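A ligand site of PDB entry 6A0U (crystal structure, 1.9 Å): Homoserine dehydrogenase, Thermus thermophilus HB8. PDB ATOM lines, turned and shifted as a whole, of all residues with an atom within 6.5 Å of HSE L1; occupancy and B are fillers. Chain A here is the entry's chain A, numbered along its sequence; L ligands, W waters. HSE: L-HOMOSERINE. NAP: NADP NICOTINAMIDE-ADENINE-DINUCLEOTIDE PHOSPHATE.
NZ of Lys 99 sits at hydrogen-bond distance from O3 of HSE L1 (2.6 Å). A nitrogen (N) of HSE L1 lies within salt-bridge range of the side-chain carboxylate (OD1) of Asp 186, 2.6 Å away. N of Gly 151 lies within hydrogen-bond range of OXT of HSE L1 (2.7 Å). A nitrogen (N) of HSE L1 lies within hydrogen-bond range of the backbone carbonyl oxygen (O) of Tyr 178, 2.7 Å away. N of Glu 180 lies close to N of HSE L1 (3.5 Å). The side-chain carboxylate of Glu 180 lies within salt-bridge range of a nitrogen (N) of HSE L1. N of Thr 152 lies within hydrogen-bond range of O of HSE L1 (2.9 Å). OG1 of Thr 152 sits at hydrogen-bond distance from O of HSE L1 (2.9 Å). ND2 of Asn 150 sits at hydrogen-bond distance from O of HSE L1 (3.3 Å). OE2 of Glu 180 is in hydrogen-bond range of O2D of NAP L2, 2.5 Å away. N of Gly 290 is in hydrogen-bond range of O7N of NAP L2, at 2.7 Å. The backbone carbonyl oxygen (O) of Gly 177 lies within hydrogen-bond range of a nitrogen (N7N) of NAP L2 (2.8 Å).
The side-chain amino group of Lys 99 is in salt-bridge range of the side-chain carboxylate of Asp 191, 2.7 Å away. The side-chain carboxylate (OD2) of Asp 186 lies within hydrogen-bond range of the backbone NH (N) of Glu 180, at 2.7 Å. N of Gly 151 sits close to ND2 of Asn 270, 3.4 Å away. OD1 of Asn 150 lies within hydrogen-bond range of N of Thr 152, 3.3 Å away. OD1 of Asn 270 is in hydrogen-bond range of N of Gly 288 (3.2 Å). The side-chain amide nitrogen (ND2) of Asn 150 sits at hydrogen-bond distance from the side-chain carboxylate (OD1) of Asp 191. The side-chain amide oxygen of Asn 150 sits at hydrogen-bond distance from the backbone NH of Thr 153. The backbone carbonyl oxygen of Asn 150 lies close to the side-chain amide nitrogen of Asn 270 (3.3 Å).
Merely in contact with HSE L1: Leu 149 (3.8 Å), Ala 179 (3.8 Å), Asp 191 (3.5 Å) and Gly 288 (3.1 Å). Within 4 Å of HSE L1: Lys 99, Leu 149, Asn 150, Gly 151, Thr 152, Tyr 178, Ala 179, Glu 180, Asp 186, Asp 191 and Gly 288. The nearest printed residue that does not touch HSE L1 is Ala 289 (4.1 Å).
Water W1 lies within hydrogen-bond range of the backbone carbonyl oxygen (O) of Leu 149, the backbone NH (N) of Met 125 and an oxygen (O3) of HSE L1.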
ATOM      1  N   ALA A  97      26.735   2.651   9.894  1.00  0.00           N
ATOM      2  CA  ALA A  97      26.312   3.984  10.145  1.00  0.00           C
ATOM      3  C   ALA A  97      24.991   4.044  11.008  1.00  0.00           C
ATOM      4  O   ALA A  97      24.451   5.107  11.185  1.00  0.00           O
ATOM      5  CB  ALA A  97      26.127   4.745   8.859  1.00  0.00           C
ATOM      6  N   LYS A  99      23.007   4.133  14.196  1.00  0.00           N
ATOM      7  CA  LYS A  99      23.122   4.420  15.658  1.00  0.00           C
ATOM      8  C   LYS A  99      21.981   3.782  16.450  1.00  0.00           C
ATOM      9  O   LYS A  99      22.171   3.315  17.594  1.00  0.00           O
ATOM     10  CB  LYS A  99      23.162   5.901  15.928  1.00  0.00           C
ATOM     11  CG  LYS A  99      21.924   6.696  15.673  1.00  0.00           C
ATOM     12  CD  LYS A  99      22.028   8.171  15.960  1.00  0.00           C
ATOM     13  CE  LYS A  99      22.537   9.051  14.831  1.00  0.00           C
ATOM     14  NZ  LYS A  99      21.755   8.933  13.552  1.00  0.00           N
ATOM     15  N   ALA A 122      30.716   6.536  11.206  1.00  0.00           N
ATOM     16  CA  ALA A 122      29.564   7.167  10.503  1.00  0.00           C
ATOM     17  C   ALA A 122      28.241   7.157  11.265  1.00  0.00           C
ATOM     18  O   ALA A 122      27.274   7.838  10.836  1.00  0.00           O
ATOM     19  CB  ALA A 122      29.366   6.561   9.056  1.00  0.00           C
ATOM     20  N   SER A 123      28.198   6.456  12.380  1.00  0.00           N
ATOM     21  CA  SER A 123      26.933   6.378  13.288  1.00  0.00           C
ATOM     22  C   SER A 123      26.744   7.673  14.140  1.00  0.00           C
ATOM     23  O   SER A 123      25.661   8.007  14.649  1.00  0.00           O
ATOM     24  CB  SER A 123      27.030   5.131  14.093  1.00  0.00           C
ATOM     25  OG  SER A 123      27.940   5.223  15.175  1.00  0.00           O
ATOM     26  N   VAL A 124      27.788   8.507  14.237  1.00  0.00           N
ATOM     27  CA  VAL A 124      27.646   9.801  14.912  1.00  0.00           C
ATOM     28  C   VAL A 124      28.288  10.912  14.156  1.00  0.00           C
ATOM     29  O   VAL A 124      29.504  10.855  13.928  1.00  0.00           O
ATOM     30  CB  VAL A 124      28.182   9.771  16.359  1.00  0.00           C
ATOM     31  CG1 VAL A 124      28.051  11.171  16.998  1.00  0.00           C
ATOM     32  CG2 VAL A 124      27.613   8.643  17.149  1.00  0.00           C
ATOM     33  N   MET A 125      27.510  11.926  13.783  1.00  0.00           N
ATOM     34  CA  MET A 125      27.925  13.025  12.992  1.00  0.00           C
ATOM     35  C   MET A 125      28.560  12.563  11.652  1.00  0.00           C
ATOM     36  O   MET A 125      29.446  13.230  11.115  1.00  0.00           O
ATOM     37  CB  MET A 125      28.886  13.941  13.765  1.00  0.00           C
ATOM     38  CG  MET A 125      28.197  14.633  14.876  1.00  0.00           C
ATOM     39  SD  MET A 125      29.249  15.487  16.062  1.00  0.00           S
ATOM     40  CE  MET A 125      30.143  16.595  15.069  1.00  0.00           C
ATOM     41  N   ALA A 126      28.038  11.474  11.108  1.00  0.00           N
ATOM     42  CA  ALA A 126      28.420  11.055   9.769  1.00  0.00           C
ATOM     43  C   ALA A 126      29.989  10.966   9.653  1.00  0.00           C
ATOM     44  O   ALA A 126      30.612  10.473  10.566  1.00  0.00           O
ATOM     45  CB  ALA A 126      27.822  11.935   8.756  1.00  0.00           C
ATOM     46  N   LEU A 149      24.255  17.045  17.966  1.00  0.00           N
ATOM     47  CA  LEU A 149      24.521  15.784  17.265  1.00  0.00           C
ATOM     48  C   LEU A 149      23.579  15.499  16.094  1.00  0.00           C
ATOM     49  O   LEU A 149      23.928  14.680  15.243  1.00  0.00           O
ATOM     50  CB  LEU A 149      24.492  14.608  18.176  1.00  0.00           C
ATOM     51  CG  LEU A 149      25.365  14.752  19.468  1.00  0.00           C
ATOM     52  CD1 LEU A 149      25.214  13.498  20.302  1.00  0.00           C
ATOM     53  CD2 LEU A 149      26.845  14.955  19.037  1.00  0.00           C
ATOM     54  N   ASN A 150      22.418  16.182  16.045  1.00  0.00           N
ATOM     55  CA  ASN A 150      21.372  15.822  15.076  1.00  0.00           C
ATOM     56  C   ASN A 150      21.390  16.870  13.999  1.00  0.00           C
ATOM     57  O   ASN A 150      21.069  18.028  14.171  1.00  0.00           O
ATOM     58  CB  ASN A 150      19.976  15.668  15.743  1.00  0.00           C
ATOM     59  CG  ASN A 150      18.911  15.212  14.741  1.00  0.00           C
ATOM     60  OD1 ASN A 150      18.277  16.025  14.177  1.00  0.00           O
ATOM     61  ND2 ASN A 150      18.870  13.971  14.479  1.00  0.00           N
ATOM     62  N   GLY A 151      21.707  16.410  12.796  1.00  0.00           N
ATOM     63  CA  GLY A 151      21.713  17.434  11.693  1.00  0.00           C
ATOM     64  C   GLY A 151      20.347  17.976  11.265  1.00  0.00           C
ATOM     65  O   GLY A 151      20.170  19.179  10.968  1.00  0.00           O
ATOM     66  N   THR A 152      19.363  17.056  11.267  1.00  0.00           N
ATOM     67  CA  THR A 152      17.980  17.485  10.873  1.00  0.00           C
ATOM     68  C   THR A 152      17.482  18.520  11.744  1.00  0.00           C
ATOM     69  O   THR A 152      17.065  19.604  11.281  1.00  0.00           O
ATOM     70  CB  THR A 152      17.080  16.269  10.859  1.00  0.00           C
ATOM     71  OG1 THR A 152      17.545  15.274   9.937  1.00  0.00           O
ATOM     72  CG2 THR A 152      15.630  16.622  10.706  1.00  0.00           C
ATOM     73  N   THR A 153      17.587  18.381  13.119  1.00  0.00           N
ATOM     74  CA  THR A 153      17.103  19.483  13.933  1.00  0.00           C
ATOM     75  C   THR A 153      17.965  20.727  13.967  1.00  0.00           C
ATOM     76  O   THR A 153      17.502  21.826  14.284  1.00  0.00           O
ATOM     77  CB  THR A 153      16.794  19.013  15.396  1.00  0.00           C
ATOM     78  OG1 THR A 153      17.884  18.256  15.935  1.00  0.00           O
ATOM     79  CG2 THR A 153      15.677  17.989  15.356  1.00  0.00           C
ATOM     80  N   GLY A 177      18.086  14.438   2.405  1.00  0.00           N
ATOM     81  CA  GLY A 177      18.507  13.068   2.754  1.00  0.00           C
ATOM     82  C   GLY A 177      19.029  13.039   4.192  1.00  0.00           C
ATOM     83  O   GLY A 177      19.533  12.005   4.632  1.00  0.00           O
ATOM     84  N   TYR A 178      18.863  14.141   4.921  1.00  0.00           N
ATOM     85  CA  TYR A 178      19.198  14.147   6.386  1.00  0.00           C
ATOM     86  C   TYR A 178      18.365  13.287   7.409  1.00  0.00           C
ATOM     87  O   TYR A 178      18.963  12.761   8.387  1.00  0.00           O
ATOM     88  CB  TYR A 178      19.170  15.559   6.931  1.00  0.00           C
ATOM     89  CG  TYR A 178      20.048  16.509   6.228  1.00  0.00           C
ATOM     90  CD1 TYR A 178      21.094  16.061   5.351  1.00  0.00           C
ATOM     91  CD2 TYR A 178      19.886  17.862   6.412  1.00  0.00           C
ATOM     92  CE1 TYR A 178      21.853  16.987   4.616  1.00  0.00           C
ATOM     93  CE2 TYR A 178      20.605  18.765   5.694  1.00  0.00           C
ATOM     94  CZ  TYR A 178      21.606  18.335   4.843  1.00  0.00           C
ATOM     95  OH  TYR A 178      22.376  19.253   4.230  1.00  0.00           O
ATOM     96  N   ALA A 179      17.026  13.145   7.199  1.00  0.00           N
ATOM     97  CA  ALA A 179      16.116  12.801   8.294  1.00  0.00           C
ATOM     98  C   ALA A 179      16.062  11.386   8.391  1.00  0.00           C
ATOM     99  O   ALA A 179      16.310  10.649   7.441  1.00  0.00           O
ATOM    100  CB  ALA A 179      14.742  13.473   8.095  1.00  0.00           C
ATOM    101  N   GLU A 180      15.851  10.891   9.585  1.00  0.00           N
ATOM    102  CA  GLU A 180      15.628   9.524   9.692  1.00  0.00           C
ATOM    103  C   GLU A 180      14.267   9.294   8.872  1.00  0.00           C
ATOM    104  O   GLU A 180      13.550  10.262   8.526  1.00  0.00           O
ATOM    105  CB  GLU A 180      15.499   9.033  11.152  1.00  0.00           C
ATOM    106  CG  GLU A 180      16.824   9.121  11.968  1.00  0.00           C
ATOM    107  CD  GLU A 180      17.935   8.389  11.222  1.00  0.00           C
ATOM    108  OE1 GLU A 180      18.702   9.115  10.643  1.00  0.00           O
ATOM    109  OE2 GLU A 180      17.972   7.113  11.238  1.00  0.00           O
ATOM    110  N   ASP A 186      14.196  12.318  14.875  1.00  0.00           N
ATOM    111  CA  ASP A 186      14.984  13.513  14.868  1.00  0.00           C
ATOM    112  C   ASP A 186      14.398  14.572  15.728  1.00  0.00           C
ATOM    113  O   ASP A 186      15.076  15.055  16.660  1.00  0.00           O
ATOM    114  CB  ASP A 186      15.235  14.076  13.453  1.00  0.00           C
ATOM    115  CG  ASP A 186      15.899  13.072  12.521  1.00  0.00           C
ATOM    116  OD1 ASP A 186      17.085  12.677  12.746  1.00  0.00           O
ATOM    117  OD2 ASP A 186      15.254  12.678  11.487  1.00  0.00           O
ATOM    118  N   ASP A 191      16.998  10.436  18.066  1.00  0.00           N
ATOM    119  CA  ASP A 191      18.158  10.138  17.273  1.00  0.00           C
ATOM    120  C   ASP A 191      19.471  10.711  17.996  1.00  0.00           C
ATOM    121  O   ASP A 191      20.450  10.004  18.129  1.00  0.00           O
ATOM    122  CB  ASP A 191      17.984  10.772  15.913  1.00  0.00           C
ATOM    123  CG  ASP A 191      19.178  10.467  14.962  1.00  0.00           C
ATOM    124  OD1 ASP A 191      20.035  11.373  14.910  1.00  0.00           O
ATOM    125  OD2 ASP A 191      19.265   9.326  14.411  1.00  0.00           O
ATOM    126  N   LYS A 195      22.706   8.717  19.582  1.00  0.00           N
ATOM    127  CA  LYS A 195      24.145   9.161  19.369  1.00  0.00           C
ATOM    128  C   LYS A 195      24.851   9.349  20.741  1.00  0.00           C
ATOM    129  O   LYS A 195      25.993   8.881  20.918  1.00  0.00           O
ATOM    130  CB  LYS A 195      24.173  10.438  18.545  1.00  0.00           C
ATOM    131  N   ASN A 270      27.081  20.196  12.593  1.00  0.00           N
ATOM    132  CA  ASN A 270      26.993  19.545  13.898  1.00  0.00           C
ATOM    133  C   ASN A 270      28.308  19.726  14.635  1.00  0.00           C
ATOM    134  O   ASN A 270      29.314  20.024  13.978  1.00  0.00           O
ATOM    135  CB  ASN A 270      26.689  18.089  13.695  1.00  0.00           C
ATOM    136  CG  ASN A 270      25.256  17.983  13.137  1.00  0.00           C
ATOM    137  OD1 ASN A 270      25.037  17.997  11.921  1.00  0.00           O
ATOM    138  ND2 ASN A 270      24.328  18.167  14.026  1.00  0.00           N
ATOM    139  N   GLY A 288      26.855  16.599   9.625  1.00  0.00           N
ATOM    140  CA  GLY A 288      26.425  15.438  10.453  1.00  0.00           C
ATOM    141  C   GLY A 288      25.400  14.482   9.869  1.00  0.00           C
ATOM    142  O   GLY A 288      25.003  13.472  10.548  1.00  0.00           O
ATOM    143  N   ALA A 289      25.101  14.723   8.600  1.00  0.00           N
ATOM    144  CA  ALA A 289      24.126  13.968   7.879  1.00  0.00           C
ATOM    145  C   ALA A 289      24.376  14.228   6.387  1.00  0.00           C
ATOM    146  O   ALA A 289      25.045  15.198   6.049  1.00  0.00           O
ATOM    147  CB  ALA A 289      22.705  14.472   8.260  1.00  0.00           C
ATOM    148  N   GLY A 290      23.813  13.368   5.510  1.00  0.00           N
ATOM    149  CA  GLY A 290      24.021  13.485   4.045  1.00  0.00           C
ATOM    150  C   GLY A 290      24.664  12.181   3.534  1.00  0.00           C
ATOM    151  O   GLY A 290      25.421  11.517   4.275  1.00  0.00           O
ATOM    152  N   THR A 294      28.174  10.706   5.023  1.00  0.00           N
ATOM    153  CA  THR A 294      28.176   9.450   5.634  1.00  0.00           C
ATOM    154  C   THR A 294      29.054   8.417   4.976  1.00  0.00           C
ATOM    155  O   THR A 294      29.766   7.628   5.677  1.00  0.00           O
ATOM    156  CB  THR A 294      26.686   8.936   5.759  1.00  0.00           C
ATOM    157  OG1 THR A 294      25.901   9.956   6.358  1.00  0.00           O
ATOM    158  CG2 THR A 294      26.584   7.832   6.567  1.00  0.00           C
HETATM  159  N   HSE L   1      18.872  11.903  10.951  1.00  0.00           N
HETATM  160  CA  HSE L   1      20.303  11.945  11.441  1.00  0.00           C
HETATM  161  C   HSE L   1      20.636  13.399  11.663  1.00  0.00           C
HETATM  162  C3  HSE L   1      21.358  11.185  10.556  1.00  0.00           C
HETATM  163  O   HSE L   1      19.807  14.212  11.313  1.00  0.00           O
HETATM  164  OXT HSE L   1      21.688  13.787  12.297  1.00  0.00           O
HETATM  165  C4  HSE L   1      22.841  11.276  11.047  1.00  0.00           C
HETATM  166  O3  HSE L   1      23.138  10.763  12.351  1.00  0.00           O
HETATM  167  PA  NAP L   2      17.570   5.069   2.797  1.00  0.00           P
HETATM  168  O1A NAP L   2      16.163   4.688   3.148  1.00  0.00           O
HETATM  169  O2A NAP L   2      17.887   6.050   1.773  1.00  0.00           O
HETATM  170  O5B NAP L   2      18.234   3.646   2.441  1.00  0.00           O
HETATM  171  C5B NAP L   2      17.821   2.429   3.088  1.00  0.00           C
HETATM  172  C4B NAP L   2      18.358   1.287   2.251  1.00  0.00           C
HETATM  173  O4B NAP L   2      18.163   0.018   2.897  1.00  0.00           O
HETATM  174  C3B NAP L   2      17.593   1.202   0.938  1.00  0.00           C
HETATM  175  O3B NAP L   2      18.408   0.685  -0.123  1.00  0.00           O
HETATM  176  C2B NAP L   2      16.449   0.211   1.218  1.00  0.00           C
HETATM  177  O2B NAP L   2      16.069  -0.529   0.054  1.00  0.00           O
HETATM  178  C1B NAP L   2      17.109  -0.729   2.202  1.00  0.00           C
HETATM  179  N9A NAP L   2      16.218  -1.283   3.212  1.00  0.00           N
HETATM  180  C8A NAP L   2      15.527  -0.584   4.181  1.00  0.00           C
HETATM  181  N7A NAP L   2      14.974  -1.500   5.034  1.00  0.00           N
HETATM  182  C5A NAP L   2      15.251  -2.757   4.580  1.00  0.00           C
HETATM  183  C6A NAP L   2      14.946  -4.177   4.945  1.00  0.00           C
HETATM  184  N6A NAP L   2      14.193  -4.525   6.001  1.00  0.00           N
HETATM  185  N1A NAP L   2      15.484  -5.169   4.207  1.00  0.00           N
HETATM  186  C2A NAP L   2      16.296  -4.910   3.147  1.00  0.00           C
HETATM  187  N3A NAP L   2      16.603  -3.664   2.717  1.00  0.00           N
HETATM  188  C4A NAP L   2      16.132  -2.570   3.395  1.00  0.00           C
HETATM  189  O3  NAP L   2      18.212   5.353   4.289  1.00  0.00           O
HETATM  190  PN  NAP L   2      19.739   5.985   4.512  1.00  0.00           P
HETATM  191  O1N NAP L   2      19.700   7.428   4.477  1.00  0.00           O
HETATM  192  O2N NAP L   2      20.660   5.396   3.428  1.00  0.00           O
HETATM  193  O5D NAP L   2      20.042   5.442   5.994  1.00  0.00           O
HETATM  194  C5D NAP L   2      20.515   4.171   6.231  1.00  0.00           C
HETATM  195  C4D NAP L   2      21.163   4.219   7.559  1.00  0.00           C
HETATM  196  O4D NAP L   2      22.170   5.190   7.477  1.00  0.00           O
HETATM  197  C3D NAP L   2      20.168   4.623   8.682  1.00  0.00           C
HETATM  198  O3D NAP L   2      20.538   3.673   9.686  1.00  0.00           O
HETATM  199  C2D NAP L   2      20.474   6.012   9.063  1.00  0.00           C
HETATM  200  O2D NAP L   2      20.168   6.170  10.447  1.00  0.00           O
HETATM  201  C1D NAP L   2      22.003   5.944   8.707  1.00  0.00           C
HETATM  202  N1N NAP L   2      22.536   7.232   8.475  1.00  0.00           N
HETATM  203  C2N NAP L   2      21.987   8.073   7.575  1.00  0.00           C
HETATM  204  C3N NAP L   2      22.520   9.305   7.422  1.00  0.00           C
HETATM  205  C7N NAP L   2      21.932  10.242   6.475  1.00  0.00           C
HETATM  206  O7N NAP L   2      22.242  11.406   6.592  1.00  0.00           O
HETATM  207  N7N NAP L   2      21.050   9.822   5.567  1.00  0.00           N
HETATM  208  C4N NAP L   2      23.665   9.706   8.180  1.00  0.00           C
HETATM  209  C5N NAP L   2      24.213   8.797   9.033  1.00  0.00           C
HETATM  210  C6N NAP L   2      23.623   7.574   9.190  1.00  0.00           C
HETATM  211  P2B NAP L   2      15.404   0.364  -1.118  1.00  0.00           P
HETATM  212  O1X NAP L   2      14.210   1.110  -0.655  1.00  0.00           O
HETATM  213  O2X NAP L   2      16.233   1.559  -1.705  1.00  0.00           O
HETATM  214  O3X NAP L   2      15.125  -0.802  -2.073  1.00  0.00           O
HETATM  215  O   HOH W   1      24.957  12.234  14.665  1.00  0.00           O
HETATM  216  O   HOH W   2      25.781   9.872  11.886  1.00  0.00           O
